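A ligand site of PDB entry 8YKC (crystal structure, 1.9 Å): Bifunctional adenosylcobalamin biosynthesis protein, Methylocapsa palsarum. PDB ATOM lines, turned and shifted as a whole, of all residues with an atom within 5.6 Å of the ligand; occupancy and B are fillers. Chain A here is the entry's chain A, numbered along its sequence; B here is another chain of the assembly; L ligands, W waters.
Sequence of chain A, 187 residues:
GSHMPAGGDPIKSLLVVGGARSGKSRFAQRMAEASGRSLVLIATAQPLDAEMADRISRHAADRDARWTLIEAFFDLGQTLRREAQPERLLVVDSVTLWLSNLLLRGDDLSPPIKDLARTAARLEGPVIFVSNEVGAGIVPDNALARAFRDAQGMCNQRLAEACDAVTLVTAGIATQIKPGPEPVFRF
An oxygen (O1) of the ligand lies close to the backbone carbonyl oxygen of Gly 19. C of Ala 20 touches O1 of the ligand (3.9 Å). CD2 of Leu 97 touches O11 of the ligand, 3.4 Å away. Val 139 of chain B touches the ligand. Arg 146 of chain B touches the ligand (CD to N4, 3.5 Å). Hydrophobic or aromatic side chains that line the ligand: Met 52, His 59, Leu 97 and Val 139 of chain B. 16 residues have an atom within 4 Å of the ligand: Gly 19, Ala 20, Arg 21, Ser 22, Gly 23, Lys 24, Ser 25, Glu 51, Met 52, Arg 55, Arg 58, His 59, Leu 97, Val 139 of chain B, Arg 146 of chain B and Asp 150 of chain B. The nearest printed residue that does not touch the ligand is Gln 157 of chain B (4.1 Å).
Water W4 lies within hydrogen-bond range of an oxygen (O3) of the ligand, the guanidinium group of Arg 21 and the side-chain amide nitrogen of Gln 157 of chain B. Water W9 lies within hydrogen-bond range of an oxygen (O10) of the ligand (2.7 Å) and the side-chain carboxylate of Glu 51 (2.7 Å). Water W8 lies within hydrogen-bond range of O3 of the ligand (2.8 Å), N of Arg 26 (2.9 Å) and N of Ser 25 (3.5 Å). Water W6 bridges O5 of the ligand (2.8 Å) and NE2 of His 59 (3.5 Å). Water W7 bridges the side-chain hydroxyl of Ser 100 (3.0 Å) and an oxygen (O11) of the ligand (3.3 Å). Water W3 lies within hydrogen-bond range of NH1 of Arg 149 of chain B (3.1 Å) and N2 of the ligand (3.3 Å).
An oxygen (O2) of the ligand lies within hydrogen-bond range of the backbone NH (N) of Ser 25 (3.1 Å). The side-chain hydroxyl (OG) of Ser 25 is in hydrogen-bond range of an oxygen (O2) of the ligand. The side-chain carboxylate (OD1) of Asp 150 of chain B sits at hydrogen-bond distance from an oxygen (O9) of the ligand (2.5 Å). A ring nitrogen (NE2) of His 59 sits at hydrogen-bond distance from an oxygen (O5) of the ligand (2.6 Å). An oxygen (O1) of the ligand is in salt-bridge range of the side-chain amino group (NZ) of Lys 24, 2.7 Å away. The guanidinium group (NH1) of Arg 58 lies within salt-bridge range of an oxygen (O5) of the ligand (2.8 Å). O3 of the ligand is in hydrogen-bond range of N of Gly 23 (2.9 Å). The backbone NH (N) of Arg 21 lies within hydrogen-bond range of an oxygen (O1) of the ligand (2.9 Å). The backbone NH of Ser 22 sits at hydrogen-bond distance from an oxygen (O1) of the ligand (2.9 Å). An oxygen (O1) of the ligand is in hydrogen-bond range of the side-chain hydroxyl (OG) of Ser 22, at 3.3 Å. An oxygen (O6) of the ligand lies within salt-bridge range of the guanidinium group (NE) of Arg 55. OE1 of Glu 51 is in hydrogen-bond range of N4 of the ligand (3.1 Å). SD of Met 52 sits close to N3 of the ligand, 3.7 Å away.
The side-chain carboxylate of Asp 150 of chain B is in salt-bridge range of the guanidinium group of Arg 21 (3.0 Å). The backbone NH (N) of Lys 24 sits at hydrogen-bond distance from the side-chain hydroxyl (OG) of Ser 22. NZ of Lys 24 sits at hydrogen-bond distance from O of Gly 19 (3.0 Å). O of Arg 21 sits at hydrogen-bond distance from NE2 of Gln 157 of chain B (2.9 Å). The side-chain hydroxyl of Ser 22 lies within hydrogen-bond range of the backbone carbonyl oxygen of Gly 19, at 2.8 Å. NE of Arg 146 of chain B is in salt-bridge range of OE1 of Glu 51 (2.7 Å). N of Glu 51 lies close to OD1 of Asp 49 (3.3 Å). The backbone NH (N) of Met 52 lies within hydrogen-bond range of the side-chain carboxylate (OD1) of Asp 49.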
ATOM      1  N   GLY A  19       6.403  34.553 -25.184  1.00  0.00           N
ATOM      2  CA  GLY A  19       6.995  34.084 -26.454  1.00  0.00           C
ATOM      3  C   GLY A  19       6.500  32.698 -26.807  1.00  0.00           C
ATOM      4  O   GLY A  19       5.646  32.105 -26.113  1.00  0.00           O
ATOM      5  N   ALA A  20       7.046  32.157 -27.882  1.00  0.00           N
ATOM      6  CA  ALA A  20       6.696  30.829 -28.366  1.00  0.00           C
ATOM      7  C   ALA A  20       7.196  29.818 -27.344  1.00  0.00           C
ATOM      8  O   ALA A  20       8.411  29.910 -26.914  1.00  0.00           O
ATOM      9  CB  ALA A  20       7.287  30.660 -29.744  1.00  0.00           C
ATOM     10  N   ARG A  21       6.324  28.880 -26.983  1.00  0.00           N
ATOM     11  CA  ARG A  21       6.678  27.760 -26.071  1.00  0.00           C
ATOM     12  C   ARG A  21       7.244  28.327 -24.759  1.00  0.00           C
ATOM     13  O   ARG A  21       8.401  27.982 -24.296  1.00  0.00           O
ATOM     14  CB  ARG A  21       7.657  26.822 -26.775  1.00  0.00           C
ATOM     15  CG  ARG A  21       7.573  25.385 -26.284  1.00  0.00           C
ATOM     16  CD  ARG A  21       6.333  24.716 -26.826  1.00  0.00           C
ATOM     17  NE  ARG A  21       6.130  23.472 -26.112  1.00  0.00           N
ATOM     18  CZ  ARG A  21       6.510  22.282 -26.530  1.00  0.00           C
ATOM     19  NH1 ARG A  21       7.101  22.136 -27.709  1.00  0.00           N
ATOM     20  NH2 ARG A  21       6.319  21.242 -25.748  1.00  0.00           N
ATOM     21  N   SER A  22       6.497  29.268 -24.208  1.00  0.00           N
ATOM     22  CA  SER A  22       6.867  30.047 -22.992  1.00  0.00           C
ATOM     23  C   SER A  22       6.208  29.444 -21.745  1.00  0.00           C
ATOM     24  O   SER A  22       6.529  29.909 -20.629  1.00  0.00           O
ATOM     25  CB  SER A  22       6.467  31.486 -23.184  1.00  0.00           C
ATOM     26  OG  SER A  22       5.051  31.565 -23.393  1.00  0.00           O
ATOM     27  N   GLY A  23       5.223  28.566 -21.907  1.00  0.00           N
ATOM     28  CA  GLY A  23       4.386  28.140 -20.778  1.00  0.00           C
ATOM     29  C   GLY A  23       3.080  28.905 -20.653  1.00  0.00           C
ATOM     30  O   GLY A  23       2.303  28.614 -19.726  1.00  0.00           O
ATOM     31  N   LYS A  24       2.817  29.870 -21.547  1.00  0.00           N
ATOM     32  CA  LYS A  24       1.638  30.755 -21.390  1.00  0.00           C
ATOM     33  C   LYS A  24       0.335  29.936 -21.413  1.00  0.00           C
ATOM     34  O   LYS A  24      -0.544  30.249 -20.572  1.00  0.00           O
ATOM     35  CB  LYS A  24       1.704  31.851 -22.441  1.00  0.00           C
ATOM     36  CG  LYS A  24       1.720  31.443 -23.893  1.00  0.00           C
ATOM     37  CD  LYS A  24       1.874  32.665 -24.791  1.00  0.00           C
ATOM     38  CE  LYS A  24       1.795  32.341 -26.277  1.00  0.00           C
ATOM     39  NZ  LYS A  24       2.831  31.387 -26.734  1.00  0.00           N
ATOM     40  N   SER A  25       0.198  28.929 -22.285  1.00  0.00           N
ATOM     41  CA  SER A  25      -1.044  28.109 -22.391  1.00  0.00           C
ATOM     42  C   SER A  25      -1.253  27.328 -21.095  1.00  0.00           C
ATOM     43  O   SER A  25      -2.390  27.324 -20.589  1.00  0.00           O
ATOM     44  CB  SER A  25      -1.044  27.164 -23.551  1.00  0.00           C
ATOM     45  OG  SER A  25      -0.832  27.837 -24.772  1.00  0.00           O
ATOM     46  N   ARG A  26      -0.183  26.718 -20.568  1.00  0.00           N
ATOM     47  CA  ARG A  26      -0.241  25.950 -19.304  1.00  0.00           C
ATOM     48  C   ARG A  26      -0.633  26.877 -18.149  1.00  0.00           C
ATOM     49  O   ARG A  26      -1.447  26.449 -17.324  1.00  0.00           O
ATOM     50  CB  ARG A  26       1.086  25.244 -19.018  1.00  0.00           C
ATOM     51  CG  ARG A  26       1.077  24.458 -17.712  1.00  0.00           C
ATOM     52  CD  ARG A  26       2.454  23.938 -17.315  1.00  0.00           C
ATOM     53  NE  ARG A  26       3.412  25.021 -17.085  1.00  0.00           N
ATOM     54  CZ  ARG A  26       4.739  24.919 -17.167  1.00  0.00           C
ATOM     55  NH1 ARG A  26       5.319  23.756 -17.441  1.00  0.00           N
ATOM     56  NH2 ARG A  26       5.495  25.987 -16.953  1.00  0.00           N
ATOM     57  N   ASP A  49      -0.893  22.110 -41.164  1.00  0.00           N
ATOM     58  CA  ASP A  49       0.246  21.209 -41.456  1.00  0.00           C
ATOM     59  C   ASP A  49       0.551  20.313 -40.256  1.00  0.00           C
ATOM     60  O   ASP A  49      -0.077  20.499 -39.197  1.00  0.00           O
ATOM     61  CB  ASP A  49       1.500  21.991 -41.881  1.00  0.00           C
ATOM     62  CG  ASP A  49       1.979  23.052 -40.898  1.00  0.00           C
ATOM     63  OD1 ASP A  49       1.780  22.896 -39.673  1.00  0.00           O
ATOM     64  OD2 ASP A  49       2.584  24.017 -41.367  1.00  0.00           O
ATOM     65  N   GLU A  51       3.068  20.275 -38.233  1.00  0.00           N
ATOM     66  CA  GLU A  51       3.587  21.032 -37.059  1.00  0.00           C
ATOM     67  C   GLU A  51       2.425  21.618 -36.257  1.00  0.00           C
ATOM     68  O   GLU A  51       2.506  21.627 -34.997  1.00  0.00           O
ATOM     69  CB  GLU A  51       4.513  22.160 -37.507  1.00  0.00           C
ATOM     70  CG  GLU A  51       5.860  21.691 -38.000  1.00  0.00           C
ATOM     71  CD  GLU A  51       6.873  22.803 -38.257  1.00  0.00           C
ATOM     72  OE1 GLU A  51       6.660  23.939 -37.753  1.00  0.00           O
ATOM     73  OE2 GLU A  51       7.893  22.521 -38.954  1.00  0.00           O
ATOM     74  N   MET A  52       1.411  22.135 -36.948  1.00  0.00           N
ATOM     75  CA  MET A  52       0.231  22.740 -36.288  1.00  0.00           C
ATOM     76  C   MET A  52      -0.575  21.621 -35.648  1.00  0.00           C
ATOM     77  O   MET A  52      -1.023  21.800 -34.509  1.00  0.00           O
ATOM     78  CB  MET A  52      -0.624  23.524 -37.283  1.00  0.00           C
ATOM     79  CG  MET A  52       0.003  24.854 -37.673  1.00  0.00           C
ATOM     80  SD  MET A  52       0.212  25.971 -36.233  1.00  0.00           S
ATOM     81  CE  MET A  52      -1.318  25.650 -35.348  1.00  0.00           C
ATOM     82  N   ARG A  55       0.958  20.574 -32.375  1.00  0.00           N
ATOM     83  CA  ARG A  55       0.660  21.561 -31.295  1.00  0.00           C
ATOM     84  C   ARG A  55      -0.773  21.285 -30.819  1.00  0.00           C
ATOM     85  O   ARG A  55      -1.023  21.288 -29.619  1.00  0.00           O
ATOM     86  CB  ARG A  55       0.824  22.993 -31.814  1.00  0.00           C
ATOM     87  CG  ARG A  55       0.570  24.041 -30.740  1.00  0.00           C
ATOM     88  CD  ARG A  55       0.260  25.426 -31.258  1.00  0.00           C
ATOM     89  NE  ARG A  55      -0.294  26.309 -30.246  1.00  0.00           N
ATOM     90  CZ  ARG A  55      -1.591  26.433 -29.951  1.00  0.00           C
ATOM     91  NH1 ARG A  55      -2.504  25.702 -30.562  1.00  0.00           N
ATOM     92  NH2 ARG A  55      -1.966  27.293 -29.038  1.00  0.00           N
ATOM     93  N   ARG A  58      -0.834  18.178 -28.581  1.00  0.00           N
ATOM     94  CA  ARG A  58      -0.264  18.481 -27.239  1.00  0.00           C
ATOM     95  C   ARG A  58      -1.328  19.209 -26.399  1.00  0.00           C
ATOM     96  O   ARG A  58      -1.500  18.846 -25.227  1.00  0.00           O
ATOM     97  CB  ARG A  58       1.038  19.255 -27.451  1.00  0.00           C
ATOM     98  CG  ARG A  58       2.036  19.175 -26.305  1.00  0.00           C
ATOM     99  CD  ARG A  58       3.421  19.643 -26.686  1.00  0.00           C
ATOM    100  NE  ARG A  58       3.560  20.615 -27.788  1.00  0.00           N
ATOM    101  CZ  ARG A  58       3.260  21.915 -27.727  1.00  0.00           C
ATOM    102  NH1 ARG A  58       2.773  22.438 -26.610  1.00  0.00           N
ATOM    103  NH2 ARG A  58       3.447  22.692 -28.784  1.00  0.00           N
ATOM    104  N   HIS A  59      -2.055  20.174 -26.964  1.00  0.00           N
ATOM    105  CA  HIS A  59      -3.031  20.997 -26.192  1.00  0.00           C
ATOM    106  C   HIS A  59      -4.222  20.119 -25.762  1.00  0.00           C
ATOM    107  O   HIS A  59      -4.606  20.208 -24.568  1.00  0.00           O
ATOM    108  CB  HIS A  59      -3.438  22.258 -26.974  1.00  0.00           C
ATOM    109  CG  HIS A  59      -2.409  23.333 -26.892  1.00  0.00           C
ATOM    110  ND1 HIS A  59      -2.749  24.662 -26.718  1.00  0.00           N
ATOM    111  CD2 HIS A  59      -1.060  23.279 -26.938  1.00  0.00           C
ATOM    112  CE1 HIS A  59      -1.632  25.384 -26.636  1.00  0.00           C
ATOM    113  NE2 HIS A  59      -0.591  24.557 -26.786  1.00  0.00           N
ATOM    114  N   LEU A  97      -2.850  33.161 -33.255  1.00  0.00           N
ATOM    115  CA  LEU A  97      -3.226  32.281 -34.416  1.00  0.00           C
ATOM    116  C   LEU A  97      -4.543  32.774 -35.039  1.00  0.00           C
ATOM    117  O   LEU A  97      -4.701  32.676 -36.252  1.00  0.00           O
ATOM    118  CB  LEU A  97      -3.291  30.823 -33.974  1.00  0.00           C
ATOM    119  CG  LEU A  97      -1.929  30.194 -33.706  1.00  0.00           C
ATOM    120  CD1 LEU A  97      -2.089  28.835 -33.037  1.00  0.00           C
ATOM    121  CD2 LEU A  97      -1.105  30.079 -34.996  1.00  0.00           C
ATOM    122  N   SER A 100      -3.360  35.394 -37.327  1.00  0.00           N
ATOM    123  CA  SER A 100      -2.673  34.711 -38.453  1.00  0.00           C
ATOM    124  C   SER A 100      -3.708  34.209 -39.471  1.00  0.00           C
ATOM    125  O   SER A 100      -3.413  34.295 -40.662  1.00  0.00           O
ATOM    126  CB  SER A 100      -1.827  33.543 -38.004  1.00  0.00           C
ATOM    127  OG  SER A 100      -0.835  33.978 -37.102  1.00  0.00           O
ATOM    128  N   VAL A 130      -4.914  34.265 -24.238  1.00  0.00           N
ATOM    129  CA  VAL A 130      -3.505  33.876 -24.383  1.00  0.00           C
ATOM    130  C   VAL A 130      -2.999  34.434 -25.717  1.00  0.00           C
ATOM    131  O   VAL A 130      -3.608  34.177 -26.782  1.00  0.00           O
ATOM    132  CB  VAL A 130      -3.310  32.346 -24.301  1.00  0.00           C
ATOM    133  CG1 VAL A 130      -1.838  32.020 -24.301  1.00  0.00           C
ATOM    134  CG2 VAL A 130      -3.988  31.758 -23.068  1.00  0.00           C
ATOM    135  N   VAL B 139       7.371  33.755 -36.290  1.00  0.00           N
ATOM    136  CA  VAL B 139       7.573  32.310 -36.581  1.00  0.00           C
ATOM    137  C   VAL B 139       8.599  32.236 -37.712  1.00  0.00           C
ATOM    138  O   VAL B 139       8.398  32.888 -38.753  1.00  0.00           O
ATOM    139  CB  VAL B 139       6.269  31.592 -36.976  1.00  0.00           C
ATOM    140  CG1 VAL B 139       6.533  30.153 -37.386  1.00  0.00           C
ATOM    141  CG2 VAL B 139       5.193  31.664 -35.909  1.00  0.00           C
ATOM    142  N   ARG B 146      12.470  26.785 -36.677  1.00  0.00           N
ATOM    143  CA  ARG B 146      11.169  26.581 -35.972  1.00  0.00           C
ATOM    144  C   ARG B 146      11.345  25.511 -34.890  1.00  0.00           C
ATOM    145  O   ARG B 146      10.839  25.730 -33.758  1.00  0.00           O
ATOM    146  CB  ARG B 146      10.042  26.219 -36.938  1.00  0.00           C
ATOM    147  CG  ARG B 146       9.360  27.416 -37.576  1.00  0.00           C
ATOM    148  CD  ARG B 146       7.954  27.140 -38.097  1.00  0.00           C
ATOM    149  NE  ARG B 146       7.960  25.997 -38.984  1.00  0.00           N
ATOM    150  CZ  ARG B 146       8.448  25.966 -40.225  1.00  0.00           C
ATOM    151  NH1 ARG B 146       9.010  27.027 -40.770  1.00  0.00           N
ATOM    152  NH2 ARG B 146       8.403  24.828 -40.894  1.00  0.00           N
ATOM    153  N   ARG B 149      13.686  26.939 -32.030  1.00  0.00           N
ATOM    154  CA  ARG B 149      12.808  27.892 -31.289  1.00  0.00           C
ATOM    155  C   ARG B 149      11.912  27.139 -30.302  1.00  0.00           C
ATOM    156  O   ARG B 149      11.877  27.533 -29.141  1.00  0.00           O
ATOM    157  CB  ARG B 149      11.943  28.683 -32.277  1.00  0.00           C
ATOM    158  CG  ARG B 149      11.158  29.831 -31.658  1.00  0.00           C
ATOM    159  CD  ARG B 149      10.564  30.609 -32.813  1.00  0.00           C
ATOM    160  NE  ARG B 149       9.630  31.725 -32.571  1.00  0.00           N
ATOM    161  CZ  ARG B 149       8.325  31.654 -32.755  1.00  0.00           C
ATOM    162  NH1 ARG B 149       7.744  30.506 -33.067  1.00  0.00           N
ATOM    163  NH2 ARG B 149       7.580  32.739 -32.618  1.00  0.00           N
ATOM    164  N   ASP B 150      11.258  26.084 -30.741  1.00  0.00           N
ATOM    165  CA  ASP B 150      10.337  25.224 -29.954  1.00  0.00           C
ATOM    166  C   ASP B 150      11.095  24.506 -28.824  1.00  0.00           C
ATOM    167  O   ASP B 150      10.668  24.556 -27.631  1.00  0.00           O
ATOM    168  CB  ASP B 150       9.605  24.291 -30.908  1.00  0.00           C
ATOM    169  CG  ASP B 150       8.377  23.638 -30.303  1.00  0.00           C
ATOM    170  OD1 ASP B 150       7.584  24.332 -29.652  1.00  0.00           O
ATOM    171  OD2 ASP B 150       8.214  22.441 -30.522  1.00  0.00           O
ATOM    172  N   GLN B 157      11.693  26.200 -19.969  1.00  0.00           N
ATOM    173  CA  GLN B 157      10.596  25.914 -19.002  1.00  0.00           C
ATOM    174  C   GLN B 157      11.060  24.801 -18.032  1.00  0.00           C
ATOM    175  O   GLN B 157      10.807  24.910 -16.808  1.00  0.00           O
ATOM    176  CB  GLN B 157       9.332  25.470 -19.730  1.00  0.00           C
ATOM    177  CG  GLN B 157       8.574  26.575 -20.442  1.00  0.00           C
ATOM    178  CD  GLN B 157       7.398  25.941 -21.145  1.00  0.00           C
ATOM    179  OE1 GLN B 157       6.497  25.381 -20.550  1.00  0.00           O
ATOM    180  NE2 GLN B 157       7.457  25.931 -22.453  1.00  0.00           N
HETATM  181  P1  LIG L   1       3.130  28.036 -25.043  1.00  0.00           P
HETATM  182  O1  LIG L   1       3.871  29.261 -25.476  1.00  0.00           O
HETATM  183  O2  LIG L   1       1.644  28.167 -24.884  1.00  0.00           O
HETATM  184  O3  LIG L   1       3.881  27.188 -24.078  1.00  0.00           O
HETATM  185  O4  LIG L   1       3.366  27.152 -26.425  1.00  0.00           O
HETATM  186  P2  LIG L   1       2.418  26.295 -27.329  1.00  0.00           P
HETATM  187  O5  LIG L   1       1.928  25.124 -26.503  1.00  0.00           O
HETATM  188  O6  LIG L   1       1.383  27.139 -27.971  1.00  0.00           O
HETATM  189  O7  LIG L   1       3.438  25.647 -28.437  1.00  0.00           O
HETATM  190  C1  LIG L   1       4.152  26.556 -29.246  1.00  0.00           C
HETATM  191  C2  LIG L   1       4.849  25.858 -30.386  1.00  0.00           C
HETATM  192  O8  LIG L   1       3.861  25.480 -31.330  1.00  0.00           O
HETATM  193  C3  LIG L   1       5.843  26.762 -31.122  1.00  0.00           C
HETATM  194  O9  LIG L   1       7.186  26.680 -30.559  1.00  0.00           O
HETATM  195  C4  LIG L   1       5.779  26.209 -32.527  1.00  0.00           C
HETATM  196  O10 LIG L   1       6.608  25.038 -32.559  1.00  0.00           O
HETATM  197  C5  LIG L   1       4.339  25.756 -32.656  1.00  0.00           C
HETATM  198  N1  LIG L   1       3.589  26.830 -33.312  1.00  0.00           N
HETATM  199  C6  LIG L   1       2.865  27.826 -32.731  1.00  0.00           C
HETATM  200  N2  LIG L   1       2.334  28.667 -33.673  1.00  0.00           N
HETATM  201  C7  LIG L   1       2.787  28.233 -34.873  1.00  0.00           C
HETATM  202  C8  LIG L   1       2.622  28.629 -36.281  1.00  0.00           C
HETATM  203  O11 LIG L   1       1.914  29.607 -36.542  1.00  0.00           O
HETATM  204  N3  LIG L   1       3.236  27.910 -37.217  1.00  0.00           N
HETATM  205  C9  LIG L   1       3.967  26.816 -36.916  1.00  0.00           C
HETATM  206  N4  LIG L   1       4.554  26.143 -37.923  1.00  0.00           N
HETATM  207  N5  LIG L   1       4.180  26.370 -35.644  1.00  0.00           N
HETATM  208  C10 LIG L   1       3.633  27.048 -34.615  1.00  0.00           C
HETATM  209  O   HOH W   1       3.503  29.915 -29.639  1.00  0.00           O
HETATM  210  O   HOH W   2       2.218  31.351 -33.269  1.00  0.00           O
HETATM  211  O   HOH W   3       4.731  30.623 -32.427  1.00  0.00           O
HETATM  212  O   HOH W   4       4.862  24.796 -23.753  1.00  0.00           O
HETATM  213  O   HOH W   5       8.846  27.628 -32.879  1.00  0.00           O
HETATM  214  O   HOH W   6       1.332  24.240 -23.939  1.00  0.00           O
HETATM  215  O   HOH W   7       1.429  32.713 -35.609  1.00  0.00           O
HETATM  216  O   HOH W   8       2.196  26.110 -22.172  1.00  0.00           O
HETATM  217  O   HOH W   9       6.634  24.021 -35.021  1.00  0.00           O
